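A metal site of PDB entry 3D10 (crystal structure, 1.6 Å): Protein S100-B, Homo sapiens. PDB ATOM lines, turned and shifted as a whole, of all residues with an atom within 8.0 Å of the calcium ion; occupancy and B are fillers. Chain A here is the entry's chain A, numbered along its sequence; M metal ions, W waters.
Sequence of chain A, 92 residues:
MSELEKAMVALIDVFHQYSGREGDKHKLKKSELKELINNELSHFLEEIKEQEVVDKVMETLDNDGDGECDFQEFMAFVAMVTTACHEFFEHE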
ATOM      1  N   PHE A  15     -29.794 -24.739 -14.266  1.00  0.00           N
ATOM      2  CA  PHE A  15     -28.408 -24.307 -14.014  1.00  0.00           C
ATOM      3  C   PHE A  15     -27.976 -23.178 -14.995  1.00  0.00           C
ATOM      4  O   PHE A  15     -27.307 -22.193 -14.632  1.00  0.00           O
ATOM      5  CB  PHE A  15     -27.390 -25.477 -14.154  1.00  0.00           C
ATOM      6  CG  PHE A  15     -25.952 -25.061 -13.895  1.00  0.00           C
ATOM      7  CD1 PHE A  15     -25.502 -24.835 -12.561  1.00  0.00           C
ATOM      8  CD2 PHE A  15     -25.038 -24.869 -14.922  1.00  0.00           C
ATOM      9  CE1 PHE A  15     -24.178 -24.457 -12.324  1.00  0.00           C
ATOM     10  CE2 PHE A  15     -23.762 -24.470 -14.675  1.00  0.00           C
ATOM     11  CZ  PHE A  15     -23.302 -24.263 -13.387  1.00  0.00           C
ATOM     12  N   HIS A  16     -28.276 -23.355 -16.281  1.00  0.00           N
ATOM     13  CA  HIS A  16     -27.741 -22.479 -17.277  1.00  0.00           C
ATOM     14  C   HIS A  16     -28.495 -21.150 -17.258  1.00  0.00           C
ATOM     15  O   HIS A  16     -27.939 -20.101 -17.559  1.00  0.00           O
ATOM     16  CB  HIS A  16     -27.961 -23.090 -18.671  1.00  0.00           C
ATOM     17  CG  HIS A  16     -26.972 -24.148 -19.059  1.00  0.00           C
ATOM     18  ND1 HIS A  16     -27.289 -25.146 -19.961  1.00  0.00           N
ATOM     19  CD2 HIS A  16     -25.662 -24.322 -18.738  1.00  0.00           C
ATOM     20  CE1 HIS A  16     -26.227 -25.914 -20.139  1.00  0.00           C
ATOM     21  NE2 HIS A  16     -25.223 -25.426 -19.418  1.00  0.00           N
ATOM     22  N   GLN A  17     -29.783 -21.227 -16.895  1.00  0.00           N
ATOM     23  CA  GLN A  17     -30.601 -20.048 -16.806  1.00  0.00           C
ATOM     24  C   GLN A  17     -29.973 -19.075 -15.818  1.00  0.00           C
ATOM     25  O   GLN A  17     -29.828 -17.855 -16.140  1.00  0.00           O
ATOM     26  CB  GLN A  17     -32.028 -20.429 -16.431  1.00  0.00           C
ATOM     27  CG  GLN A  17     -32.760 -20.920 -17.632  1.00  0.00           C
ATOM     28  CD  GLN A  17     -33.958 -21.772 -17.349  1.00  0.00           C
ATOM     29  OE1 GLN A  17     -34.471 -21.842 -16.230  1.00  0.00           O
ATOM     30  NE2 GLN A  17     -34.416 -22.471 -18.396  1.00  0.00           N
ATOM     31  N   TYR A  18     -29.548 -19.636 -14.677  1.00  0.00           N
ATOM     32  CA  TYR A  18     -28.983 -18.822 -13.585  1.00  0.00           C
ATOM     33  C   TYR A  18     -27.505 -18.545 -13.707  1.00  0.00           C
ATOM     34  O   TYR A  18     -27.072 -17.445 -13.361  1.00  0.00           O
ATOM     35  CB  TYR A  18     -29.369 -19.363 -12.187  1.00  0.00           C
ATOM     36  CG  TYR A  18     -30.866 -19.130 -11.949  1.00  0.00           C
ATOM     37  CD1 TYR A  18     -31.792 -20.087 -12.266  1.00  0.00           C
ATOM     38  CD2 TYR A  18     -31.301 -17.934 -11.379  1.00  0.00           C
ATOM     39  CE1 TYR A  18     -33.209 -19.803 -12.123  1.00  0.00           C
ATOM     40  CE2 TYR A  18     -32.659 -17.664 -11.201  1.00  0.00           C
ATOM     41  CZ  TYR A  18     -33.591 -18.594 -11.539  1.00  0.00           C
ATOM     42  OH  TYR A  18     -34.933 -18.230 -11.330  1.00  0.00           O
ATOM     43  N   SER A  19     -26.725 -19.534 -14.177  1.00  0.00           N
ATOM     44  CA  SER A  19     -25.255 -19.319 -14.332  1.00  0.00           C
ATOM     45  C   SER A  19     -24.817 -18.313 -15.433  1.00  0.00           C
ATOM     46  O   SER A  19     -23.791 -17.646 -15.299  1.00  0.00           O
ATOM     47  CB  SER A  19     -24.556 -20.679 -14.490  1.00  0.00           C
ATOM     48  OG  SER A  19     -24.776 -21.221 -15.796  1.00  0.00           O
ATOM     49  N   GLY A  20     -25.553 -18.246 -16.547  1.00  0.00           N
ATOM     50  CA  GLY A  20     -25.239 -17.343 -17.618  1.00  0.00           C
ATOM     51  C   GLY A  20     -25.665 -15.899 -17.386  1.00  0.00           C
ATOM     52  O   GLY A  20     -25.613 -15.103 -18.299  1.00  0.00           O
ATOM     53  N   ARG A  21     -26.102 -15.563 -16.175  1.00  0.00           N
ATOM     54  CA  ARG A  21     -26.573 -14.196 -15.917  1.00  0.00           C
ATOM     55  C   ARG A  21     -25.450 -13.195 -15.814  1.00  0.00           C
ATOM     56  O   ARG A  21     -25.526 -12.097 -16.391  1.00  0.00           O
ATOM     57  CB  ARG A  21     -27.427 -14.169 -14.644  1.00  0.00           C
ATOM     58  CG  ARG A  21     -28.857 -14.677 -14.833  1.00  0.00           C
ATOM     59  CD  ARG A  21     -29.624 -14.640 -13.503  1.00  0.00           C
ATOM     60  NE  ARG A  21     -30.999 -15.031 -13.679  1.00  0.00           N
ATOM     61  CZ  ARG A  21     -31.996 -14.773 -12.834  1.00  0.00           C
ATOM     62  NH1 ARG A  21     -33.243 -15.186 -13.115  1.00  0.00           N
ATOM     63  NH2 ARG A  21     -31.782 -14.056 -11.748  1.00  0.00           N
ATOM     64  N   GLU A  22     -24.401 -13.555 -15.085  1.00  0.00           N
ATOM     65  CA  GLU A  22     -23.222 -12.691 -14.990  1.00  0.00           C
ATOM     66  C   GLU A  22     -21.919 -13.473 -14.798  1.00  0.00           C
ATOM     67  O   GLU A  22     -21.932 -14.636 -14.378  1.00  0.00           O
ATOM     68  CB  GLU A  22     -23.349 -11.673 -13.850  1.00  0.00           C
ATOM     69  CG  GLU A  22     -24.710 -11.556 -13.187  1.00  0.00           C
ATOM     70  CD  GLU A  22     -24.636 -10.751 -11.892  1.00  0.00           C
ATOM     71  OE1 GLU A  22     -25.411  -9.780 -11.737  1.00  0.00           O
ATOM     72  OE2 GLU A  22     -23.760 -11.080 -11.038  1.00  0.00           O
ATOM     73  N   GLY A  23     -20.798 -12.821 -15.091  1.00  0.00           N
ATOM     74  CA  GLY A  23     -19.499 -13.430 -14.923  1.00  0.00           C
ATOM     75  C   GLY A  23     -19.293 -14.666 -15.783  1.00  0.00           C
ATOM     76  O   GLY A  23     -19.651 -14.661 -16.958  1.00  0.00           O
ATOM     77  N   ASP A  24     -18.686 -15.697 -15.176  1.00  0.00           N
ATOM     78  CA  ASP A  24     -18.502 -17.018 -15.791  1.00  0.00           C
ATOM     79  C   ASP A  24     -19.874 -17.510 -16.133  1.00  0.00           C
ATOM     80  O   ASP A  24     -20.668 -17.788 -15.242  1.00  0.00           O
ATOM     81  CB  ASP A  24     -17.863 -18.021 -14.806  1.00  0.00           C
ATOM     82  CG  ASP A  24     -17.387 -19.306 -15.479  1.00  0.00           C
ATOM     83  OD1 ASP A  24     -18.135 -19.882 -16.248  1.00  0.00           O
ATOM     84  OD2 ASP A  24     -16.214 -19.712 -15.298  1.00  0.00           O
ATOM     85  N   LYS A  25     -20.182 -17.601 -17.430  1.00  0.00           N
ATOM     86  CA  LYS A  25     -21.522 -18.048 -17.789  1.00  0.00           C
ATOM     87  C   LYS A  25     -21.866 -19.486 -17.379  1.00  0.00           C
ATOM     88  O   LYS A  25     -22.997 -19.923 -17.565  1.00  0.00           O
ATOM     89  CB  LYS A  25     -21.811 -17.843 -19.262  1.00  0.00           C
ATOM     90  CG  LYS A  25     -21.993 -16.387 -19.597  1.00  0.00           C
ATOM     91  CD  LYS A  25     -22.607 -16.196 -20.967  1.00  0.00           C
ATOM     92  CE  LYS A  25     -22.985 -14.741 -21.173  1.00  0.00           C
ATOM     93  NZ  LYS A  25     -21.848 -13.771 -21.226  1.00  0.00           N
ATOM     94  N   HIS A  26     -20.881 -20.226 -16.874  1.00  0.00           N
ATOM     95  CA  HIS A  26     -21.027 -21.645 -16.549  1.00  0.00           C
ATOM     96  C   HIS A  26     -20.845 -21.895 -15.035  1.00  0.00           C
ATOM     97  O   HIS A  26     -20.607 -23.028 -14.604  1.00  0.00           O
ATOM     98  CB  HIS A  26     -19.978 -22.442 -17.336  1.00  0.00           C
ATOM     99  CG  HIS A  26     -20.512 -23.656 -18.039  1.00  0.00           C
ATOM    100  ND1 HIS A  26     -19.690 -24.684 -18.455  1.00  0.00           N
ATOM    101  CD2 HIS A  26     -21.768 -24.000 -18.418  1.00  0.00           C
ATOM    102  CE1 HIS A  26     -20.429 -25.608 -19.055  1.00  0.00           C
ATOM    103  NE2 HIS A  26     -21.689 -25.224 -19.018  1.00  0.00           N
ATOM    104  N   LYS A  27     -20.898 -20.844 -14.226  1.00  0.00           N
ATOM    105  CA  LYS A  27     -20.848 -20.991 -12.786  1.00  0.00           C
ATOM    106  C   LYS A  27     -21.854 -20.088 -12.130  1.00  0.00           C
ATOM    107  O   LYS A  27     -22.047 -18.987 -12.648  1.00  0.00           O
ATOM    108  CB  LYS A  27     -19.449 -20.696 -12.229  1.00  0.00           C
ATOM    109  CG  LYS A  27     -18.283 -21.571 -12.764  1.00  0.00           C
ATOM    110  CD  LYS A  27     -17.138 -21.488 -11.740  1.00  0.00           C
ATOM    111  CE  LYS A  27     -15.775 -21.430 -12.398  1.00  0.00           C
ATOM    112  NZ  LYS A  27     -15.381 -22.686 -13.081  1.00  0.00           N
ATOM    113  N   LEU A  28     -22.431 -20.533 -10.991  1.00  0.00           N
ATOM    114  CA  LEU A  28     -23.321 -19.712 -10.144  1.00  0.00           C
ATOM    115  C   LEU A  28     -22.526 -18.877  -9.153  1.00  0.00           C
ATOM    116  O   LEU A  28     -21.877 -19.417  -8.299  1.00  0.00           O
ATOM    117  CB  LEU A  28     -24.302 -20.583  -9.314  1.00  0.00           C
ATOM    118  CG  LEU A  28     -25.285 -21.383 -10.153  1.00  0.00           C
ATOM    119  CD1 LEU A  28     -25.941 -22.551  -9.350  1.00  0.00           C
ATOM    120  CD2 LEU A  28     -26.350 -20.561 -10.933  1.00  0.00           C
ATOM    121  N   LYS A  29     -22.561 -17.559  -9.290  1.00  0.00           N
ATOM    122  CA  LYS A  29     -22.090 -16.738  -8.196  1.00  0.00           C
ATOM    123  C   LYS A  29     -23.212 -16.580  -7.140  1.00  0.00           C
ATOM    124  O   LYS A  29     -24.412 -16.979  -7.374  1.00  0.00           O
ATOM    125  CB  LYS A  29     -21.523 -15.382  -8.675  1.00  0.00           C
ATOM    126  CG  LYS A  29     -22.568 -14.429  -9.255  1.00  0.00           C
ATOM    127  CD  LYS A  29     -21.945 -13.243 -10.076  1.00  0.00           C
ATOM    128  CE  LYS A  29     -20.832 -12.564  -9.363  1.00  0.00           C
ATOM    129  NZ  LYS A  29     -19.517 -13.205  -9.616  1.00  0.00           N
ATOM    130  N   LYS A  30     -22.850 -15.961  -6.004  1.00  0.00           N
ATOM    131  CA  LYS A  30     -23.749 -15.905  -4.863  1.00  0.00           C
ATOM    132  C   LYS A  30     -25.115 -15.311  -5.223  1.00  0.00           C
ATOM    133  O   LYS A  30     -26.165 -15.855  -4.848  1.00  0.00           O
ATOM    134  CB  LYS A  30     -23.140 -15.115  -3.735  1.00  0.00           C
ATOM    135  CG  LYS A  30     -21.867 -15.717  -3.280  1.00  0.00           C
ATOM    136  CD  LYS A  30     -21.514 -15.136  -1.964  1.00  0.00           C
ATOM    137  CE  LYS A  30     -20.712 -16.180  -1.210  1.00  0.00           C
ATOM    138  NZ  LYS A  30     -20.123 -15.544  -0.009  1.00  0.00           N
ATOM    139  N   SER A  31     -25.107 -14.239  -5.993  1.00  0.00           N
ATOM    140  CA  SER A  31     -26.364 -13.661  -6.323  1.00  0.00           C
ATOM    141  C   SER A  31     -27.224 -14.560  -7.250  1.00  0.00           C
ATOM    142  O   SER A  31     -28.430 -14.579  -7.124  1.00  0.00           O
ATOM    143  CB  SER A  31     -26.215 -12.243  -6.912  1.00  0.00           C
ATOM    144  OG  SER A  31     -25.521 -12.286  -8.122  1.00  0.00           O
ATOM    145  N   GLU A  32     -26.598 -15.303  -8.164  1.00  0.00           N
ATOM    146  CA  GLU A  32     -27.363 -16.176  -9.060  1.00  0.00           C
ATOM    147  C   GLU A  32     -27.920 -17.340  -8.301  1.00  0.00           C
ATOM    148  O   GLU A  32     -29.028 -17.835  -8.510  1.00  0.00           O
ATOM    149  CB  GLU A  32     -26.493 -16.642 -10.215  1.00  0.00           C
ATOM    150  CG  GLU A  32     -26.177 -15.560 -11.220  1.00  0.00           C
ATOM    151  CD  GLU A  32     -24.984 -15.900 -11.969  1.00  0.00           C
ATOM    152  OE1 GLU A  32     -24.286 -16.858 -11.505  1.00  0.00           O
ATOM    153  OE2 GLU A  32     -24.688 -15.230 -12.983  1.00  0.00           O
ATOM    154  N   LEU A  33     -27.079 -17.868  -7.430  1.00  0.00           N
ATOM    155  CA  LEU A  33     -27.476 -18.929  -6.520  1.00  0.00           C
ATOM    156  C   LEU A  33     -28.687 -18.501  -5.666  1.00  0.00           C
ATOM    157  O   LEU A  33     -29.647 -19.244  -5.581  1.00  0.00           O
ATOM    158  CB  LEU A  33     -26.295 -19.289  -5.633  1.00  0.00           C
ATOM    159  CG  LEU A  33     -26.468 -20.512  -4.725  1.00  0.00           C
ATOM    160  CD1 LEU A  33     -27.148 -21.784  -5.365  1.00  0.00           C
ATOM    161  CD2 LEU A  33     -25.111 -20.915  -4.073  1.00  0.00           C
ATOM    162  N   GLU A  68     -17.643 -19.947  -6.208  1.00  0.00           N
ATOM    163  CA  GLU A  68     -18.763 -20.103  -7.123  1.00  0.00           C
ATOM    164  C   GLU A  68     -19.225 -21.570  -7.146  1.00  0.00           C
ATOM    165  O   GLU A  68     -18.549 -22.487  -6.711  1.00  0.00           O
ATOM    166  CB  GLU A  68     -18.414 -19.646  -8.551  1.00  0.00           C
ATOM    167  CG  GLU A  68     -17.875 -18.209  -8.631  1.00  0.00           C
ATOM    168  CD  GLU A  68     -18.462 -17.390  -9.757  1.00  0.00           C
ATOM    169  OE1 GLU A  68     -19.441 -17.819 -10.437  1.00  0.00           O
ATOM    170  OE2 GLU A  68     -17.950 -16.254  -9.910  1.00  0.00           O
ATOM    171  N   CYS A  69     -20.400 -21.782  -7.649  1.00  0.00           N
ATOM    172  CA  CYS A  69     -20.935 -23.145  -7.768  1.00  0.00           C
ATOM    173  C   CYS A  69     -20.870 -23.562  -9.226  1.00  0.00           C
ATOM    174  O   CYS A  69     -21.576 -22.952 -10.052  1.00  0.00           O
ATOM    175  CB  CYS A  69     -22.415 -23.148  -7.392  1.00  0.00           C
ATOM    176  SG  CYS A  69     -23.149 -24.772  -7.299  1.00  0.00           S
HETATM  177 CA    CA M   1     -22.508 -16.739 -13.601  1.00  0.00          CA
HETATM  178  O   HOH W   1     -20.840 -16.194 -12.014  1.00  0.00           O
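The side-chain hydroxyl (OG) of Ser 19 is in hydrogen-bond range of the backbone carbonyl oxygen (O) of Phe 15 (3.0 Å). N of His 26 lies within hydrogen-bond range of OD1 of Asp 24 (2.8 Å). OE1 of Glu 32 sits close to N of Lys 29 (2.9 Å). OD2 of Asp 24 is in salt-bridge range of NZ of Lys 27 (3.8 Å). The side-chain hydroxyl (OG) of Ser 19 lies within hydrogen-bond range of the backbone carbonyl oxygen (O) of Lys 25 (2.8 Å).
Within 4 Å of the calcium ion: Ser 19, Glu 22, Asp 24, Lys 27 and Glu 32. The nearest printed residue that does not touch the calcium ion is Lys 29 (4.4 Å).
The calcium ion is bound by O of Ser 19, O of Glu 22, water W1, O of Lys 27, O of Asp 24, OE2 of Glu 32 and OE1 of Glu 32. The calcium ion has seven donor atoms within binding distance.
Water W1 bridges the side-chain carboxylate (OE1) of Glu 68 (2.7 Å) and the backbone NH (N) of Lys 29 (3.5 Å).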
